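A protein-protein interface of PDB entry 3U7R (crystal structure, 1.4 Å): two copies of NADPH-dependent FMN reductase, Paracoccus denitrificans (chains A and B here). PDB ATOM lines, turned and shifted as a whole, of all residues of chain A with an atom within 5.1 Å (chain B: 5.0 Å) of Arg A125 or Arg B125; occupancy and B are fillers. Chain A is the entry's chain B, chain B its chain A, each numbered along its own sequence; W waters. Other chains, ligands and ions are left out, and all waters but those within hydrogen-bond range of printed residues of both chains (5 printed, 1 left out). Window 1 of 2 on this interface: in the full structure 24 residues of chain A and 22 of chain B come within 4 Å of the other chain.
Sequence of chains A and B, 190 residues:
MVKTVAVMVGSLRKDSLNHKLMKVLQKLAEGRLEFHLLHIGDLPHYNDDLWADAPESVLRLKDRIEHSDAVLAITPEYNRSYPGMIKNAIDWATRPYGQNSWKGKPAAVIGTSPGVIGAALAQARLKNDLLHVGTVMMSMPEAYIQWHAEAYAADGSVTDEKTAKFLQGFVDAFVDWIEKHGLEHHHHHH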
ATOM      1  N   ARG A  80       6.797 -22.860  13.648  1.00  0.00           N
ATOM      2  CA  ARG A  80       5.829 -21.747  13.682  1.00  0.00           C
ATOM      3  C   ARG A  80       4.390 -22.146  13.835  1.00  0.00           C
ATOM      4  O   ARG A  80       3.493 -21.312  13.653  1.00  0.00           O
ATOM      5  CB  ARG A  80       6.033 -20.767  12.509  1.00  0.00           C
ATOM      6  CG  ARG A  80       7.461 -20.250  12.369  1.00  0.00           C
ATOM      7  CD  ARG A  80       8.024 -19.657  13.636  1.00  0.00           C
ATOM      8  NE  ARG A  80       9.393 -19.214  13.475  1.00  0.00           N
ATOM      9  CZ  ARG A  80      10.177 -18.807  14.469  1.00  0.00           C
ATOM     10  NH1 ARG A  80       9.731 -18.724  15.701  1.00  0.00           N
ATOM     11  NH2 ARG A  80      11.426 -18.462  14.192  1.00  0.00           N
ATOM     12  N   SER A  81       4.149 -23.387  14.289  1.00  0.00           N
ATOM     13  CA  SER A  81       2.862 -23.754  14.795  1.00  0.00           C
ATOM     14  C   SER A  81       3.062 -24.741  15.937  1.00  0.00           C
ATOM     15  O   SER A  81       4.174 -24.885  16.436  1.00  0.00           O
ATOM     16  CB  SER A  81       1.966 -24.290  13.692  1.00  0.00           C
ATOM     17  OG  SER A  81       0.612 -24.426  14.180  1.00  0.00           O
ATOM     18  N   TYR A  82       2.018 -25.369  16.402  1.00  0.00           N
ATOM     19  CA  TYR A  82       2.084 -26.265  17.540  1.00  0.00           C
ATOM     20  C   TYR A  82       2.236 -27.703  17.043  1.00  0.00           C
ATOM     21  O   TYR A  82       2.050 -28.006  15.865  1.00  0.00           O
ATOM     22  CB  TYR A  82       0.859 -26.082  18.446  1.00  0.00           C
ATOM     23  CG  TYR A  82      -0.465 -26.498  17.898  1.00  0.00           C
ATOM     24  CD1 TYR A  82      -0.988 -27.757  18.170  1.00  0.00           C
ATOM     25  CD2 TYR A  82      -1.243 -25.634  17.146  1.00  0.00           C
ATOM     26  CE1 TYR A  82      -2.212 -28.178  17.690  1.00  0.00           C
ATOM     27  CE2 TYR A  82      -2.474 -26.055  16.636  1.00  0.00           C
ATOM     28  CZ  TYR A  82      -2.965 -27.324  16.930  1.00  0.00           C
ATOM     29  OH  TYR A  82      -4.185 -27.753  16.481  1.00  0.00           O
ATOM     30  N   LEU A 121       3.477 -18.028  17.971  1.00  0.00           N
ATOM     31  CA  LEU A 121       2.777 -18.496  16.743  1.00  0.00           C
ATOM     32  C   LEU A 121       2.059 -19.828  16.958  1.00  0.00           C
ATOM     33  O   LEU A 121       0.950 -20.026  16.480  1.00  0.00           O
ATOM     34  CB  LEU A 121       3.726 -18.552  15.535  1.00  0.00           C
ATOM     35  CG  LEU A 121       4.050 -17.135  14.964  1.00  0.00           C
ATOM     36  CD1 LEU A 121       5.030 -16.375  15.832  1.00  0.00           C
ATOM     37  CD2 LEU A 121       4.612 -17.183  13.581  1.00  0.00           C
ATOM     38  N   ALA A 122       2.692 -20.755  17.683  1.00  0.00           N
ATOM     39  CA  ALA A 122       2.043 -22.007  18.066  1.00  0.00           C
ATOM     40  C   ALA A 122       0.797 -21.705  18.875  1.00  0.00           C
ATOM     41  O   ALA A 122      -0.246 -22.325  18.693  1.00  0.00           O
ATOM     42  CB  ALA A 122       3.026 -22.851  18.857  1.00  0.00           C
ATOM     43  N   GLN A 123       0.914 -20.782  19.828  1.00  0.00           N
ATOM     44  CA  GLN A 123      -0.199 -20.495  20.722  1.00  0.00           C
ATOM     45  C   GLN A 123      -1.390 -19.923  19.985  1.00  0.00           C
ATOM     46  O   GLN A 123      -2.528 -20.270  20.279  1.00  0.00           O
ATOM     47  CB  GLN A 123       0.249 -19.578  21.876  1.00  0.00           C
ATOM     48  CG  GLN A 123       1.235 -20.243  22.803  1.00  0.00           C
ATOM     49  CD  GLN A 123       1.462 -19.424  24.046  1.00  0.00           C
ATOM     50  OE1 GLN A 123       0.488 -19.045  24.688  1.00  0.00           O
ATOM     51  NE2 GLN A 123       2.697 -19.156  24.393  1.00  0.00           N
ATOM     52  N   ALA A 124      -1.138 -19.029  19.056  1.00  0.00           N
ATOM     53  CA  ALA A 124      -2.234 -18.442  18.326  1.00  0.00           C
ATOM     54  C   ALA A 124      -2.983 -19.496  17.549  1.00  0.00           C
ATOM     55  O   ALA A 124      -4.240 -19.510  17.529  1.00  0.00           O
ATOM     56  CB  ALA A 124      -1.711 -17.346  17.367  1.00  0.00           C
ATOM     57  N   ARG A 125      -2.256 -20.394  16.914  1.00  0.00           N
ATOM     58  CA  ARG A 125      -2.899 -21.465  16.144  1.00  0.00           C
ATOM     59  C   ARG A 125      -3.667 -22.442  17.038  1.00  0.00           C
ATOM     60  O   ARG A 125      -4.772 -22.904  16.690  1.00  0.00           O
ATOM     61  CB  ARG A 125      -1.853 -22.199  15.334  1.00  0.00           C
ATOM     62  CG  ARG A 125      -1.231 -21.456  14.179  1.00  0.00           C
ATOM     63  CD  ARG A 125      -1.484 -19.995  13.970  1.00  0.00           C
ATOM     64  NE  ARG A 125      -1.010 -19.517  12.673  1.00  0.00           N
ATOM     65  CZ  ARG A 125       0.216 -19.618  12.141  1.00  0.00           C
ATOM     66  NH1 ARG A 125       1.244 -20.209  12.722  1.00  0.00           N
ATOM     67  NH2 ARG A 125       0.396 -19.149  10.935  1.00  0.00           N
ATOM     68  N   LEU A 126      -3.121 -22.739  18.206  1.00  0.00           N
ATOM     69  CA  LEU A 126      -3.762 -23.661  19.113  1.00  0.00           C
ATOM     70  C   LEU A 126      -5.001 -23.057  19.737  1.00  0.00           C
ATOM     71  O   LEU A 126      -6.011 -23.719  19.890  1.00  0.00           O
ATOM     72  CB  LEU A 126      -2.766 -24.108  20.164  1.00  0.00           C
ATOM     73  CG  LEU A 126      -3.289 -25.115  21.183  1.00  0.00           C
ATOM     74  CD1 LEU A 126      -3.996 -26.283  20.530  1.00  0.00           C
ATOM     75  CD2 LEU A 126      -2.143 -25.591  22.026  1.00  0.00           C
ATOM     76  N   LYS A 127      -4.937 -21.781  20.087  1.00  0.00           N
ATOM     77  CA  LYS A 127      -6.152 -21.045  20.506  1.00  0.00           C
ATOM     78  C   LYS A 127      -7.231 -21.139  19.449  1.00  0.00           C
ATOM     79  O   LYS A 127      -8.385 -21.440  19.768  1.00  0.00           O
ATOM     80  CB  LYS A 127      -5.835 -19.585  20.830  1.00  0.00           C
ATOM     81  CG  LYS A 127      -5.002 -19.424  22.098  1.00  0.00           C
ATOM     82  CD  LYS A 127      -4.530 -17.994  22.256  1.00  0.00           C
ATOM     83  CE  LYS A 127      -3.596 -17.835  23.428  1.00  0.00           C
ATOM     84  NZ  LYS A 127      -2.841 -16.541  23.346  1.00  0.00           N
ATOM     85  N   ASN A 128      -6.883 -20.919  18.187  1.00  0.00           N
ATOM     86  CA  ASN A 128      -7.890 -20.998  17.119  1.00  0.00           C
ATOM     87  C   ASN A 128      -8.476 -22.386  16.986  1.00  0.00           C
ATOM     88  O   ASN A 128      -9.694 -22.542  16.854  1.00  0.00           O
ATOM     89  CB  ASN A 128      -7.243 -20.616  15.800  1.00  0.00           C
ATOM     90  CG  ASN A 128      -8.128 -20.821  14.651  1.00  0.00           C
ATOM     91  OD1 ASN A 128      -8.147 -21.894  13.993  1.00  0.00           O
ATOM     92  ND2 ASN A 128      -8.857 -19.831  14.366  1.00  0.00           N
ATOM     93  N   ASP A 129      -7.628 -23.396  17.005  1.00  0.00           N
ATOM     94  CA  ASP A 129      -8.099 -24.768  16.800  1.00  0.00           C
ATOM     95  C   ASP A 129      -8.945 -25.279  17.958  1.00  0.00           C
ATOM     96  O   ASP A 129      -9.916 -25.985  17.748  1.00  0.00           O
ATOM     97  CB  ASP A 129      -6.923 -25.701  16.501  1.00  0.00           C
ATOM     98  CG  ASP A 129      -6.333 -25.472  15.111  1.00  0.00           C
ATOM     99  OD1 ASP A 129      -6.902 -24.713  14.272  1.00  0.00           O
ATOM    100  OD2 ASP A 129      -5.258 -26.043  14.845  1.00  0.00           O
ATOM    101  N   LEU A 130      -8.601 -24.888  19.188  1.00  0.00           N
ATOM    102  CA  LEU A 130      -9.415 -25.241  20.354  1.00  0.00           C
ATOM    103  C   LEU A 130     -10.734 -24.438  20.360  1.00  0.00           C
ATOM    104  O   LEU A 130     -11.787 -24.944  20.751  1.00  0.00           O
ATOM    105  CB  LEU A 130      -8.666 -25.071  21.666  1.00  0.00           C
ATOM    106  CG  LEU A 130      -7.741 -26.230  21.992  1.00  0.00           C
ATOM    107  CD1 LEU A 130      -6.782 -25.865  23.103  1.00  0.00           C
ATOM    108  CD2 LEU A 130      -8.525 -27.472  22.337  1.00  0.00           C
ATOM    109  N   ARG B  80     -11.788 -28.295  11.090  1.00  0.00           N
ATOM    110  CA  ARG B  80     -11.423 -27.053  10.394  1.00  0.00           C
ATOM    111  C   ARG B  80      -9.926 -26.800  10.257  1.00  0.00           C
ATOM    112  O   ARG B  80      -9.540 -25.687   9.901  1.00  0.00           O
ATOM    113  CB  ARG B  80     -12.194 -25.838  10.912  1.00  0.00           C
ATOM    114  CG  ARG B  80     -13.702 -26.052  10.991  1.00  0.00           C
ATOM    115  CD  ARG B  80     -14.299 -26.443   9.660  1.00  0.00           C
ATOM    116  NE  ARG B  80     -15.733 -26.630   9.765  1.00  0.00           N
ATOM    117  CZ  ARG B  80     -16.482 -27.184   8.809  1.00  0.00           C
ATOM    118  NH1 ARG B  80     -15.945 -27.533   7.670  1.00  0.00           N
ATOM    119  NH2 ARG B  80     -17.789 -27.351   9.042  1.00  0.00           N
ATOM    120  N   SER B  81      -9.119 -27.843  10.475  1.00  0.00           N
ATOM    121  CA  SER B  81      -7.728 -27.826  10.022  1.00  0.00           C
ATOM    122  C   SER B  81      -7.326 -29.189   9.549  1.00  0.00           C
ATOM    123  O   SER B  81      -8.200 -30.014   9.330  1.00  0.00           O
ATOM    124  CB  SER B  81      -6.831 -27.249  11.119  1.00  0.00           C
ATOM    125  OG  SER B  81      -5.537 -27.004  10.610  1.00  0.00           O
ATOM    126  N   TYR B  82      -6.048 -29.420   9.327  1.00  0.00           N
ATOM    127  CA  TYR B  82      -5.585 -30.694   8.795  1.00  0.00           C
ATOM    128  C   TYR B  82      -5.136 -31.605   9.939  1.00  0.00           C
ATOM    129  O   TYR B  82      -5.008 -31.177  11.086  1.00  0.00           O
ATOM    130  CB  TYR B  82      -4.488 -30.476   7.778  1.00  0.00           C
ATOM    131  CG  TYR B  82      -3.189 -29.904   8.303  1.00  0.00           C
ATOM    132  CD1 TYR B  82      -2.147 -30.767   8.636  1.00  0.00           C
ATOM    133  CD2 TYR B  82      -2.977 -28.526   8.415  1.00  0.00           C
ATOM    134  CE1 TYR B  82      -0.930 -30.300   9.049  1.00  0.00           C
ATOM    135  CE2 TYR B  82      -1.760 -28.056   8.889  1.00  0.00           C
ATOM    136  CZ  TYR B  82      -0.748 -28.948   9.206  1.00  0.00           C
ATOM    137  OH  TYR B  82       0.492 -28.501   9.651  1.00  0.00           O
ATOM    138  N   LEU B 121     -10.387 -25.366   4.566  1.00  0.00           N
ATOM    139  CA  LEU B 121      -9.769 -24.769   5.762  1.00  0.00           C
ATOM    140  C   LEU B 121      -8.513 -25.558   6.110  1.00  0.00           C
ATOM    141  O   LEU B 121      -7.483 -24.992   6.464  1.00  0.00           O
ATOM    142  CB  LEU B 121     -10.704 -24.640   6.956  1.00  0.00           C
ATOM    143  CG  LEU B 121     -11.668 -23.447   6.786  1.00  0.00           C
ATOM    144  CD1 LEU B 121     -12.761 -23.728   5.762  1.00  0.00           C
ATOM    145  CD2 LEU B 121     -12.354 -23.071   8.062  1.00  0.00           C
ATOM    146  N   ALA B 122      -8.570 -26.899   6.035  1.00  0.00           N
ATOM    147  CA  ALA B 122      -7.389 -27.725   6.212  1.00  0.00           C
ATOM    148  C   ALA B 122      -6.326 -27.356   5.220  1.00  0.00           C
ATOM    149  O   ALA B 122      -5.142 -27.259   5.574  1.00  0.00           O
ATOM    150  CB  ALA B 122      -7.787 -29.187   6.071  1.00  0.00           C
ATOM    151  N   GLN B 123      -6.702 -27.208   3.956  1.00  0.00           N
ATOM    152  CA  GLN B 123      -5.713 -26.935   2.897  1.00  0.00           C
ATOM    153  C   GLN B 123      -5.017 -25.608   3.101  1.00  0.00           C
ATOM    154  O   GLN B 123      -3.825 -25.512   2.890  1.00  0.00           O
ATOM    155  CB  GLN B 123      -6.381 -27.036   1.529  1.00  0.00           C
ATOM    156  CG  GLN B 123      -6.838 -28.427   1.186  1.00  0.00           C
ATOM    157  CD  GLN B 123      -7.236 -28.543  -0.259  1.00  0.00           C
ATOM    158  OE1 GLN B 123      -6.492 -28.123  -1.125  1.00  0.00           O
ATOM    159  NE2 GLN B 123      -8.425 -29.075  -0.523  1.00  0.00           N
ATOM    160  N   ALA B 124      -5.750 -24.584   3.520  1.00  0.00           N
ATOM    161  CA  ALA B 124      -5.148 -23.265   3.717  1.00  0.00           C
ATOM    162  C   ALA B 124      -4.087 -23.342   4.796  1.00  0.00           C
ATOM    163  O   ALA B 124      -3.003 -22.799   4.670  1.00  0.00           O
ATOM    164  CB  ALA B 124      -6.207 -22.242   4.089  1.00  0.00           C
ATOM    165  N   ARG B 125      -4.386 -24.060   5.878  1.00  0.00           N
ATOM    166  CA  ARG B 125      -3.453 -24.190   7.020  1.00  0.00           C
ATOM    167  C   ARG B 125      -2.249 -25.027   6.637  1.00  0.00           C
ATOM    168  O   ARG B 125      -1.114 -24.742   7.019  1.00  0.00           O
ATOM    169  CB  ARG B 125      -4.181 -24.828   8.181  1.00  0.00           C
ATOM    170  CG  ARG B 125      -5.228 -23.993   8.882  1.00  0.00           C
ATOM    171  CD  ARG B 125      -4.695 -22.817   9.610  1.00  0.00           C
ATOM    172  NE  ARG B 125      -3.991 -23.324  10.784  1.00  0.00           N
ATOM    173  CZ  ARG B 125      -4.580 -23.717  11.908  1.00  0.00           C
ATOM    174  NH1 ARG B 125      -5.888 -23.605  12.079  1.00  0.00           N
ATOM    175  NH2 ARG B 125      -3.845 -24.209  12.887  1.00  0.00           N
ATOM    176  N   LEU B 126      -2.471 -26.091   5.858  1.00  0.00           N
ATOM    177  CA  LEU B 126      -1.371 -26.929   5.452  1.00  0.00           C
ATOM    178  C   LEU B 126      -0.431 -26.231   4.460  1.00  0.00           C
ATOM    179  O   LEU B 126       0.769 -26.351   4.525  1.00  0.00           O
ATOM    180  CB  LEU B 126      -1.918 -28.223   4.873  1.00  0.00           C
ATOM    181  CG  LEU B 126      -0.888 -29.260   4.438  1.00  0.00           C
ATOM    182  CD1 LEU B 126       0.190 -29.512   5.475  1.00  0.00           C
ATOM    183  CD2 LEU B 126      -1.601 -30.533   4.067  1.00  0.00           C
ATOM    184  N   LYS B 127      -1.006 -25.471   3.539  1.00  0.00           N
ATOM    185  CA  LYS B 127      -0.211 -24.609   2.645  1.00  0.00           C
ATOM    186  C   LYS B 127       0.671 -23.675   3.471  1.00  0.00           C
ATOM    187  O   LYS B 127       1.857 -23.560   3.207  1.00  0.00           O
ATOM    188  CB  LYS B 127      -1.082 -23.831   1.680  1.00  0.00           C
ATOM    189  CG  LYS B 127      -1.742 -24.691   0.614  1.00  0.00           C
ATOM    190  CD  LYS B 127      -2.772 -23.917  -0.196  1.00  0.00           C
ATOM    191  CE  LYS B 127      -3.526 -24.792  -1.173  1.00  0.00           C
ATOM    192  NZ  LYS B 127      -4.776 -24.102  -1.636  1.00  0.00           N
ATOM    193  N   ASN B 128       0.101 -22.996   4.470  1.00  0.00           N
ATOM    194  CA  ASN B 128       0.883 -22.102   5.312  1.00  0.00           C
ATOM    195  C   ASN B 128       1.995 -22.829   6.053  1.00  0.00           C
ATOM    196  O   ASN B 128       3.126 -22.346   6.088  1.00  0.00           O
ATOM    197  CB  ASN B 128      -0.038 -21.516   6.353  1.00  0.00           C
ATOM    198  CG  ASN B 128       0.686 -20.663   7.331  1.00  0.00           C
ATOM    199  OD1 ASN B 128       1.125 -21.117   8.412  1.00  0.00           O
ATOM    200  ND2 ASN B 128       0.862 -19.471   6.987  1.00  0.00           N
ATOM    201  N   ASP B 129       1.691 -23.978   6.633  1.00  0.00           N
ATOM    202  CA  ASP B 129       2.699 -24.708   7.443  1.00  0.00           C
ATOM    203  C   ASP B 129       3.795 -25.290   6.588  1.00  0.00           C
ATOM    204  O   ASP B 129       4.954 -25.276   6.992  1.00  0.00           O
ATOM    205  CB  ASP B 129       2.030 -25.768   8.305  1.00  0.00           C
ATOM    206  CG  ASP B 129       1.234 -25.183   9.457  1.00  0.00           C
ATOM    207  OD1 ASP B 129       1.312 -23.958   9.705  1.00  0.00           O
ATOM    208  OD2 ASP B 129       0.469 -25.945  10.113  1.00  0.00           O
ATOM    209  N   LEU B 130       3.467 -25.747   5.387  1.00  0.00           N
ATOM    210  CA  LEU B 130       4.517 -26.197   4.467  1.00  0.00           C
ATOM    211  C   LEU B 130       5.333 -25.032   3.891  1.00  0.00           C
ATOM    212  O   LEU B 130       6.548 -25.154   3.656  1.00  0.00           O
ATOM    213  CB  LEU B 130       3.951 -27.034   3.333  1.00  0.00           C
ATOM    214  CG  LEU B 130       3.672 -28.481   3.758  1.00  0.00           C
ATOM    215  CD1 LEU B 130       2.773 -29.191   2.737  1.00  0.00           C
ATOM    216  CD2 LEU B 130       4.963 -29.268   3.949  1.00  0.00           C
HETATM  217  O   HOH W   1      -2.133 -20.602   9.160  1.00  0.00           O
HETATM  218  O   HOH W   2       3.087 -19.929  10.457  1.00  0.00           O
HETATM  219  O   HOH W   3      -1.008 -25.527  12.487  1.00  0.00           O
HETATM  220  O   HOH W   4      -0.564 -17.743   8.789  1.00  0.00           O
HETATM  221  O   HOH W   5      -5.444 -20.395  12.790  1.00  0.00           O
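Among the printed residues, 4 pairs touch across the chains. Among the printed residues, Asp or Glu carboxylates within 4 Å of a Lys or Arg side-chain nitrogen of the other chain: Asp A129 with Arg B125.
Of the printed residues of chain B, Arg A125 touches Arg B125 (3.7 Å) and Asn B128 (3.3 Å). Printed residues of chain B within 4 Å of Asn A128: Arg B125. Of the printed residues of chain B, Asp A129 touches Arg B125 (2.7 Å). Of the printed residues of chain A, Arg B125 touches Arg A125 (3.7 Å), Asn A128 (3.4 Å) and Asp A129 (2.7 Å). Printed residues of chain A within 4 Å of Asn B128: Arg A125. The nearest printed residue of chain B that does not touch Asn A128 is Arg B80 (5.8 Å).
Among the printed residues, merely in contact across the chains: Arg A125 with Arg B125 (3.7 Å).
Arg A125 touches its own counterpart, Arg B125. Arg A125 touches Asn B128, and with the chains exchanged Asn A128 touches Arg B125. Asp A129 touches Arg B125, but with the chains exchanged Arg A125 does not touch Asp B129 (4.8 Å). 13 positions are printed for both chains.
OD1 of Asp A129 is in salt-bridge range of NH1 of Arg B125 (2.7 Å). The guanidinium group of Arg B125 lies within hydrogen-bond range of the side-chain amide oxygen of Asn A128 (3.4 Å). The guanidinium group (NH2) of Arg A125 sits at hydrogen-bond distance from the side-chain amide oxygen (OD1) of Asn B128, at 3.3 Å.
The side-chain amide oxygen (OD1) of Asn B128 sits close to the side-chain carboxylate (OD1) of Asp B129 (3.1 Å). The side-chain carboxylate (OD2) of Asp A129 lies within hydrogen-bond range of the side-chain hydroxyl (OH) of Tyr A82 (2.6 Å). O of Arg A80 sits at hydrogen-bond distance from NH1 of Arg A125, 2.7 Å away. The side-chain amide oxygen of Asn A128 sits close to the side-chain carboxylate of Asp A129 (3.1 Å).
Water W3 lies within hydrogen-bond range of OG of Ser A81 (2.6 Å), OD2 of Asp B129 (2.8 Å) and NH2 of Arg B125 (3.2 Å). Water W4 bridges the guanidinium group (NH2) of Arg A125 (2.7 Å) and the side-chain amide nitrogen (ND2) of Asn B128 (2.9 Å). Water W2 lies within hydrogen-bond range of the guanidinium group of Arg A125 (2.8 Å) and the side-chain amide oxygen of Asn B128 (3.1 Å). Water W5 bridges the side-chain amide oxygen (OD1) of Asn A128 (3.3 Å) and the guanidinium group (NH1) of Arg B125 (3.3 Å). Water W1 lies within hydrogen-bond range of OD1 of Asn B128 (3.4 Å) and NH2 of Arg A125 (3.4 Å).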
